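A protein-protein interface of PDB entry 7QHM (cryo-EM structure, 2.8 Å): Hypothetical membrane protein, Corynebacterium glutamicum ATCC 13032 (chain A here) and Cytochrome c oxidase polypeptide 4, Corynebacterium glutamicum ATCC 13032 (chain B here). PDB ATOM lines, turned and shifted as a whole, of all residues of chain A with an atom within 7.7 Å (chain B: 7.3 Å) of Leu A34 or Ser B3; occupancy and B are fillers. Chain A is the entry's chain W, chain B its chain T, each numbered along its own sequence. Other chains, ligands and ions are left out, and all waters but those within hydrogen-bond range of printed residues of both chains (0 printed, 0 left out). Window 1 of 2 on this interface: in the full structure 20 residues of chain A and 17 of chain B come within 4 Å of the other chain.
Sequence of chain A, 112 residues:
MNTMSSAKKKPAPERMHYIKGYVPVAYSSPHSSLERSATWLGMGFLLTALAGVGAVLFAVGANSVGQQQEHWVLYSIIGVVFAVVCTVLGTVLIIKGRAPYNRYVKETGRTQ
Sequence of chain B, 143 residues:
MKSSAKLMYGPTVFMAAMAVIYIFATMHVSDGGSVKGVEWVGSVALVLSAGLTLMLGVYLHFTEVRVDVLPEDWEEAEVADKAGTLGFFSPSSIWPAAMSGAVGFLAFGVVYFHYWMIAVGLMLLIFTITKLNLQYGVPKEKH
Of the 17 printed residues of chain A, 4 touch a printed residue of chain B. Of the 9 printed residues of chain B, 4 touch a printed residue of chain A. Printed residues of chain B that touch a printed residue of chain A: Lys B2, Ser B3, Lys B6 and Leu B7. Hydrophobic or aromatic side chains of chain B within 4 Å of the printed part of chain A: Leu B7.
Of the printed residues of chain B, Leu A34 touches Ser B3. Of the printed residues of chain B, Glu A35 touches Lys B2 (3.5 Å), Ser B3 (3.9 Å) and Lys B6 (3.2 Å). Of the printed residues of chain B, Ser A37 touches Lys B6 (3.5 Å). Of the printed residues of chain B, Trp A40 touches Lys B6 and Leu B7. Met B1 touches none of the printed residues of chain A. Ser B3 touches just these residues of chain A: Leu A34 (3.2 Å) and Glu A35 (3.9 Å). Of the printed residues of chain A, Leu B7 touches Trp A40 (3.5 Å). The nearest residue of chain B that does not touch Leu A34 is Lys B6 (5.5 Å). The nearest residue of chain A that does not touch Ser B3 is Trp A40 (4.7 Å). The nearest printed residue of chain B that does not touch Glu A35 is Ser B4 (7.1 Å).
The backbone carbonyl oxygen of Leu A34 is in hydrogen-bond range of the indole nitrogen of Trp A40 (3.1 Å).
The backbone carbonyl oxygen of Leu A34 lies within hydrogen-bond range of the side-chain hydroxyl of Ser B3, at 3.2 Å. The side-chain carboxylate (OE2) of Glu A35 lies within salt-bridge range of the side-chain amino group (NZ) of Lys B2, at 3.5 Å. O of Glu A35 sits at hydrogen-bond distance from NZ of Lys B6 (3.2 Å).
Ser B3 touches Glu A35 (OG to CB, 3.9 Å). CG of Lys B6 touches CA of Ser A37, at 3.5 Å. Trp A40 touches Lys B6 (CB to O, 3.4 Å). Leu B7 touches Trp A40.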
ATOM      1  N   ALA A  26      12.448 -13.630   9.544  1.00  0.00           N
ATOM      2  CA  ALA A  26      11.749 -12.419   9.117  1.00  0.00           C
ATOM      3  C   ALA A  26      12.367 -11.191   9.784  1.00  0.00           C
ATOM      4  O   ALA A  26      11.732 -10.534  10.611  1.00  0.00           O
ATOM      5  CB  ALA A  26      10.265 -12.525   9.436  1.00  0.00           C
ATOM      6  N   TYR A  27      13.599 -10.862   9.396  1.00  0.00           N
ATOM      7  CA  TYR A  27      14.248  -9.652   9.882  1.00  0.00           C
ATOM      8  C   TYR A  27      13.912  -8.431   9.036  1.00  0.00           C
ATOM      9  O   TYR A  27      13.723  -7.343   9.578  1.00  0.00           O
ATOM     10  CB  TYR A  27      15.763  -9.842   9.915  1.00  0.00           C
ATOM     11  CG  TYR A  27      16.227 -10.857  10.922  1.00  0.00           C
ATOM     12  CD1 TYR A  27      16.054 -10.641  12.277  1.00  0.00           C
ATOM     13  CD2 TYR A  27      16.853 -12.020  10.521  1.00  0.00           C
ATOM     14  CE1 TYR A  27      16.467 -11.556  13.193  1.00  0.00           C
ATOM     15  CE2 TYR A  27      17.278 -12.938  11.431  1.00  0.00           C
ATOM     16  CZ  TYR A  27      17.086 -12.702  12.767  1.00  0.00           C
ATOM     17  OH  TYR A  27      17.508 -13.628  13.685  1.00  0.00           O
ATOM     18  N   SER A  28      13.843  -8.582   7.719  1.00  0.00           N
ATOM     19  CA  SER A  28      13.582  -7.470   6.818  1.00  0.00           C
ATOM     20  C   SER A  28      12.098  -7.296   6.512  1.00  0.00           C
ATOM     21  O   SER A  28      11.752  -6.675   5.503  1.00  0.00           O
ATOM     22  CB  SER A  28      14.366  -7.657   5.517  1.00  0.00           C
ATOM     23  OG  SER A  28      15.761  -7.661   5.758  1.00  0.00           O
ATOM     24  N   SER A  29      11.216  -7.822   7.356  1.00  0.00           N
ATOM     25  CA  SER A  29       9.797  -7.677   7.114  1.00  0.00           C
ATOM     26  C   SER A  29       9.386  -6.215   7.290  1.00  0.00           C
ATOM     27  O   SER A  29      10.136  -5.421   7.855  1.00  0.00           O
ATOM     28  CB  SER A  29       9.005  -8.580   8.051  1.00  0.00           C
ATOM     29  OG  SER A  29       9.542  -8.545   9.354  1.00  0.00           O
ATOM     30  N   HIS A  31       7.308  -4.806   9.272  1.00  0.00           N
ATOM     31  CA  HIS A  31       7.060  -4.434  10.658  1.00  0.00           C
ATOM     32  C   HIS A  31       8.292  -4.572  11.540  1.00  0.00           C
ATOM     33  O   HIS A  31       8.183  -4.417  12.758  1.00  0.00           O
ATOM     34  CB  HIS A  31       5.932  -5.284  11.240  1.00  0.00           C
ATOM     35  CG  HIS A  31       6.226  -6.749  11.251  1.00  0.00           C
ATOM     36  ND1 HIS A  31       6.993  -7.350  12.224  1.00  0.00           N
ATOM     37  CD2 HIS A  31       5.867  -7.731  10.397  1.00  0.00           C
ATOM     38  CE1 HIS A  31       7.087  -8.641  11.974  1.00  0.00           C
ATOM     39  NE2 HIS A  31       6.410  -8.899  10.870  1.00  0.00           N
ATOM     40  N   SER A  32       9.454  -4.855  10.967  1.00  0.00           N
ATOM     41  CA  SER A  32      10.658  -5.064  11.754  1.00  0.00           C
ATOM     42  C   SER A  32      11.384  -3.746  11.996  1.00  0.00           C
ATOM     43  O   SER A  32      11.636  -2.982  11.063  1.00  0.00           O
ATOM     44  CB  SER A  32      11.578  -6.062  11.061  1.00  0.00           C
ATOM     45  OG  SER A  32      11.086  -7.383  11.226  1.00  0.00           O
ATOM     46  N   SER A  33      11.704  -3.490  13.263  1.00  0.00           N
ATOM     47  CA  SER A  33      12.430  -2.310  13.706  1.00  0.00           C
ATOM     48  C   SER A  33      13.807  -2.156  13.080  1.00  0.00           C
ATOM     49  O   SER A  33      14.382  -1.067  13.165  1.00  0.00           O
ATOM     50  CB  SER A  33      12.564  -2.356  15.224  1.00  0.00           C
ATOM     51  OG  SER A  33      12.974  -3.637  15.649  1.00  0.00           O
ATOM     52  N   LEU A  34      14.348  -3.182  12.451  1.00  0.00           N
ATOM     53  CA  LEU A  34      15.617  -3.027  11.745  1.00  0.00           C
ATOM     54  C   LEU A  34      15.503  -2.183  10.486  1.00  0.00           C
ATOM     55  O   LEU A  34      16.504  -2.130   9.772  1.00  0.00           O
ATOM     56  CB  LEU A  34      16.185  -4.403  11.391  1.00  0.00           C
ATOM     57  CG  LEU A  34      16.588  -5.301  12.556  1.00  0.00           C
ATOM     58  CD1 LEU A  34      16.857  -6.703  12.062  1.00  0.00           C
ATOM     59  CD2 LEU A  34      17.806  -4.761  13.255  1.00  0.00           C
ATOM     60  N   GLU A  35      14.372  -1.549  10.167  1.00  0.00           N
ATOM     61  CA  GLU A  35      14.271  -0.652   9.031  1.00  0.00           C
ATOM     62  C   GLU A  35      13.572   0.665   9.348  1.00  0.00           C
ATOM     63  O   GLU A  35      13.423   1.493   8.444  1.00  0.00           O
ATOM     64  CB  GLU A  35      13.531  -1.345   7.875  1.00  0.00           C
ATOM     65  CG  GLU A  35      12.124  -1.849   8.214  1.00  0.00           C
ATOM     66  CD  GLU A  35      11.270  -2.043   6.979  1.00  0.00           C
ATOM     67  OE1 GLU A  35      11.701  -2.772   6.063  1.00  0.00           O
ATOM     68  OE2 GLU A  35      10.171  -1.453   6.915  1.00  0.00           O
ATOM     69  N   ARG A  36      13.152   0.892  10.592  1.00  0.00           N
ATOM     70  CA  ARG A  36      12.262   2.000  10.913  1.00  0.00           C
ATOM     71  C   ARG A  36      12.995   3.264  11.346  1.00  0.00           C
ATOM     72  O   ARG A  36      12.346   4.188  11.847  1.00  0.00           O
ATOM     73  CB  ARG A  36      11.267   1.578  12.002  1.00  0.00           C
ATOM     74  CG  ARG A  36      10.479   0.307  11.690  1.00  0.00           C
ATOM     75  CD  ARG A  36       9.588   0.425  10.445  1.00  0.00           C
ATOM     76  NE  ARG A  36       8.470   1.345  10.661  1.00  0.00           N
ATOM     77  CZ  ARG A  36       7.174   1.054  10.572  1.00  0.00           C
ATOM     78  NH1 ARG A  36       6.740  -0.143  10.198  1.00  0.00           N
ATOM     79  NH2 ARG A  36       6.281   1.996  10.856  1.00  0.00           N
ATOM     80  N   SER A  37      14.319   3.320  11.187  1.00  0.00           N
ATOM     81  CA  SER A  37      15.102   4.551  11.293  1.00  0.00           C
ATOM     82  C   SER A  37      15.269   5.053  12.723  1.00  0.00           C
ATOM     83  O   SER A  37      16.366   5.470  13.102  1.00  0.00           O
ATOM     84  CB  SER A  37      14.487   5.658  10.435  1.00  0.00           C
ATOM     85  OG  SER A  37      15.350   6.775  10.375  1.00  0.00           O
ATOM     86  N   THR A  39      15.238   3.140  15.294  1.00  0.00           N
ATOM     87  CA  THR A  39      16.096   2.152  15.939  1.00  0.00           C
ATOM     88  C   THR A  39      17.571   2.495  15.779  1.00  0.00           C
ATOM     89  O   THR A  39      18.323   2.485  16.754  1.00  0.00           O
ATOM     90  CB  THR A  39      15.807   0.767  15.368  1.00  0.00           C
ATOM     91  OG1 THR A  39      14.392   0.574  15.282  1.00  0.00           O
ATOM     92  CG2 THR A  39      16.399  -0.316  16.252  1.00  0.00           C
ATOM     93  N   TRP A  40      18.006   2.815  14.562  1.00  0.00           N
ATOM     94  CA  TRP A  40      19.432   3.022  14.335  1.00  0.00           C
ATOM     95  C   TRP A  40      19.938   4.305  14.989  1.00  0.00           C
ATOM     96  O   TRP A  40      21.085   4.359  15.449  1.00  0.00           O
ATOM     97  CB  TRP A  40      19.711   3.009  12.837  1.00  0.00           C
ATOM     98  CG  TRP A  40      19.391   1.691  12.199  1.00  0.00           C
ATOM     99  CD1 TRP A  40      18.223   1.332  11.605  1.00  0.00           C
ATOM    100  CD2 TRP A  40      20.252   0.555  12.101  1.00  0.00           C
ATOM    101  NE1 TRP A  40      18.301   0.049  11.137  1.00  0.00           N
ATOM    102  CE2 TRP A  40      19.540  -0.451  11.428  1.00  0.00           C
ATOM    103  CE3 TRP A  40      21.561   0.293  12.510  1.00  0.00           C
ATOM    104  CZ2 TRP A  40      20.088  -1.697  11.160  1.00  0.00           C
ATOM    105  CZ3 TRP A  40      22.102  -0.938  12.244  1.00  0.00           C
ATOM    106  CH2 TRP A  40      21.369  -1.921  11.574  1.00  0.00           C
ATOM    107  N   MET A  43      20.451   3.314  18.492  1.00  0.00           N
ATOM    108  CA  MET A  43      21.698   2.565  18.590  1.00  0.00           C
ATOM    109  C   MET A  43      22.888   3.512  18.656  1.00  0.00           C
ATOM    110  O   MET A  43      23.808   3.320  19.463  1.00  0.00           O
ATOM    111  CB  MET A  43      21.820   1.616  17.396  1.00  0.00           C
ATOM    112  CG  MET A  43      20.760   0.538  17.355  1.00  0.00           C
ATOM    113  SD  MET A  43      20.529  -0.291  15.763  1.00  0.00           S
ATOM    114  CE  MET A  43      21.798  -1.552  15.778  1.00  0.00           C
ATOM    115  N   GLY A  97      11.119   2.669  17.649  1.00  0.00           N
ATOM    116  CA  GLY A  97      11.379   1.795  16.517  1.00  0.00           C
ATOM    117  C   GLY A  97      10.720   0.433  16.656  1.00  0.00           C
ATOM    118  O   GLY A  97      10.270  -0.148  15.669  1.00  0.00           O
ATOM    119  N   ARG A  98      10.643  -0.089  17.878  1.00  0.00           N
ATOM    120  CA  ARG A  98      10.115  -1.423  18.132  1.00  0.00           C
ATOM    121  C   ARG A  98       8.611  -1.448  18.383  1.00  0.00           C
ATOM    122  O   ARG A  98       8.069  -2.519  18.666  1.00  0.00           O
ATOM    123  CB  ARG A  98      10.837  -2.040  19.330  1.00  0.00           C
ATOM    124  CG  ARG A  98      11.289  -3.468  19.117  1.00  0.00           C
ATOM    125  CD  ARG A  98      11.786  -4.089  20.395  1.00  0.00           C
ATOM    126  NE  ARG A  98      10.692  -4.315  21.336  1.00  0.00           N
ATOM    127  CZ  ARG A  98      10.632  -3.903  22.600  1.00  0.00           C
ATOM    128  NH1 ARG A  98      11.631  -3.256  23.182  1.00  0.00           N
ATOM    129  NH2 ARG A  98       9.536  -4.159  23.308  1.00  0.00           N
ATOM    130  N   TYR A 101       6.505  -3.757  15.589  1.00  0.00           N
ATOM    131  CA  TYR A 101       6.680  -5.180  15.834  1.00  0.00           C
ATOM    132  C   TYR A 101       5.890  -5.624  17.054  1.00  0.00           C
ATOM    133  O   TYR A 101       5.362  -6.739  17.087  1.00  0.00           O
ATOM    134  CB  TYR A 101       8.161  -5.505  16.013  1.00  0.00           C
ATOM    135  CG  TYR A 101       8.401  -6.896  16.537  1.00  0.00           C
ATOM    136  CD1 TYR A 101       8.228  -7.997  15.725  1.00  0.00           C
ATOM    137  CD2 TYR A 101       8.788  -7.105  17.843  1.00  0.00           C
ATOM    138  CE1 TYR A 101       8.434  -9.255  16.195  1.00  0.00           C
ATOM    139  CE2 TYR A 101       8.994  -8.359  18.319  1.00  0.00           C
ATOM    140  CZ  TYR A 101       8.818  -9.436  17.492  1.00  0.00           C
ATOM    141  OH  TYR A 101       9.031 -10.707  17.969  1.00  0.00           O
ATOM    142  N   MET B   1      15.746  -0.342  -0.414  1.00  0.00           N
ATOM    143  CA  MET B   1      17.038  -0.318   0.327  1.00  0.00           C
ATOM    144  C   MET B   1      16.883   0.446   1.632  1.00  0.00           C
ATOM    145  O   MET B   1      17.550   1.450   1.868  1.00  0.00           O
ATOM    146  CB  MET B   1      18.130   0.302  -0.535  1.00  0.00           C
ATOM    147  CG  MET B   1      17.681   1.516  -1.326  1.00  0.00           C
ATOM    148  SD  MET B   1      19.033   2.549  -1.912  1.00  0.00           S
ATOM    149  CE  MET B   1      20.142   1.338  -2.629  1.00  0.00           C
ATOM    150  N   LYS B   2      15.993  -0.050   2.489  1.00  0.00           N
ATOM    151  CA  LYS B   2      15.654   0.674   3.707  1.00  0.00           C
ATOM    152  C   LYS B   2      16.744   0.533   4.761  1.00  0.00           C
ATOM    153  O   LYS B   2      17.271   1.534   5.258  1.00  0.00           O
ATOM    154  CB  LYS B   2      14.319   0.176   4.250  1.00  0.00           C
ATOM    155  CG  LYS B   2      13.117   0.708   3.499  1.00  0.00           C
ATOM    156  CD  LYS B   2      11.817   0.334   4.195  1.00  0.00           C
ATOM    157  CE  LYS B   2      10.627   1.038   3.569  1.00  0.00           C
ATOM    158  NZ  LYS B   2       9.355   0.699   4.260  1.00  0.00           N
ATOM    159  N   SER B   3      17.098  -0.705   5.101  1.00  0.00           N
ATOM    160  CA  SER B   3      18.040  -0.945   6.184  1.00  0.00           C
ATOM    161  C   SER B   3      19.405  -0.349   5.882  1.00  0.00           C
ATOM    162  O   SER B   3      20.069   0.182   6.778  1.00  0.00           O
ATOM    163  CB  SER B   3      18.152  -2.441   6.431  1.00  0.00           C
ATOM    164  OG  SER B   3      16.872  -2.990   6.683  1.00  0.00           O
ATOM    165  N   SER B   4      19.833  -0.407   4.623  1.00  0.00           N
ATOM    166  CA  SER B   4      21.115   0.170   4.245  1.00  0.00           C
ATOM    167  C   SER B   4      21.122   1.677   4.458  1.00  0.00           C
ATOM    168  O   SER B   4      22.073   2.235   5.015  1.00  0.00           O
ATOM    169  CB  SER B   4      21.425  -0.168   2.789  1.00  0.00           C
ATOM    170  OG  SER B   4      22.688   0.334   2.407  1.00  0.00           O
ATOM    171  N   ALA B   5      20.069   2.358   4.015  1.00  0.00           N
ATOM    172  CA  ALA B   5      20.007   3.802   4.194  1.00  0.00           C
ATOM    173  C   ALA B   5      19.921   4.166   5.668  1.00  0.00           C
ATOM    174  O   ALA B   5      20.505   5.164   6.103  1.00  0.00           O
ATOM    175  CB  ALA B   5      18.812   4.373   3.436  1.00  0.00           C
ATOM    176  N   LYS B   6      19.212   3.363   6.455  1.00  0.00           N
ATOM    177  CA  LYS B   6      18.952   3.737   7.835  1.00  0.00           C
ATOM    178  C   LYS B   6      20.125   3.431   8.754  1.00  0.00           C
ATOM    179  O   LYS B   6      20.332   4.157   9.731  1.00  0.00           O
ATOM    180  CB  LYS B   6      17.683   3.046   8.337  1.00  0.00           C
ATOM    181  CG  LYS B   6      16.410   3.871   8.144  1.00  0.00           C
ATOM    182  CD  LYS B   6      16.055   4.076   6.680  1.00  0.00           C
ATOM    183  CE  LYS B   6      14.838   4.959   6.513  1.00  0.00           C
ATOM    184  NZ  LYS B   6      13.574   4.218   6.750  1.00  0.00           N
ATOM    185  N   LEU B   7      20.915   2.397   8.472  1.00  0.00           N
ATOM    186  CA  LEU B   7      22.031   2.070   9.355  1.00  0.00           C
ATOM    187  C   LEU B   7      23.213   3.018   9.213  1.00  0.00           C
ATOM    188  O   LEU B   7      24.200   2.851   9.931  1.00  0.00           O
ATOM    189  CB  LEU B   7      22.498   0.630   9.123  1.00  0.00           C
ATOM    190  CG  LEU B   7      23.145   0.220   7.797  1.00  0.00           C
ATOM    191  CD1 LEU B   7      24.642   0.466   7.757  1.00  0.00           C
ATOM    192  CD2 LEU B   7      22.872  -1.241   7.539  1.00  0.00           C
ATOM    193  N   MET B   8      23.157   3.987   8.306  1.00  0.00           N
ATOM    194  CA  MET B   8      24.178   5.021   8.229  1.00  0.00           C
ATOM    195  C   MET B   8      23.989   6.125   9.259  1.00  0.00           C
ATOM    196  O   MET B   8      24.828   7.025   9.327  1.00  0.00           O
ATOM    197  CB  MET B   8      24.188   5.640   6.834  1.00  0.00           C
ATOM    198  CG  MET B   8      24.954   4.852   5.811  1.00  0.00           C
ATOM    199  SD  MET B   8      26.731   4.981   6.045  1.00  0.00           S
ATOM    200  CE  MET B   8      27.298   4.098   4.596  1.00  0.00           C
ATOM    201  N   GLU B  64      15.478   5.972  -1.454  1.00  0.00           N
ATOM    202  CA  GLU B  64      14.610   4.919  -0.931  1.00  0.00           C
ATOM    203  C   GLU B  64      13.152   5.348  -0.853  1.00  0.00           C
ATOM    204  O   GLU B  64      12.253   4.527  -1.061  1.00  0.00           O
ATOM    205  CB  GLU B  64      15.111   4.503   0.454  1.00  0.00           C
ATOM    206  CG  GLU B  64      14.133   3.708   1.323  1.00  0.00           C
ATOM    207  CD  GLU B  64      13.609   2.463   0.642  1.00  0.00           C
ATOM    208  OE1 GLU B  64      14.361   1.864  -0.158  1.00  0.00           O
ATOM    209  OE2 GLU B  64      12.449   2.082   0.905  1.00  0.00           O
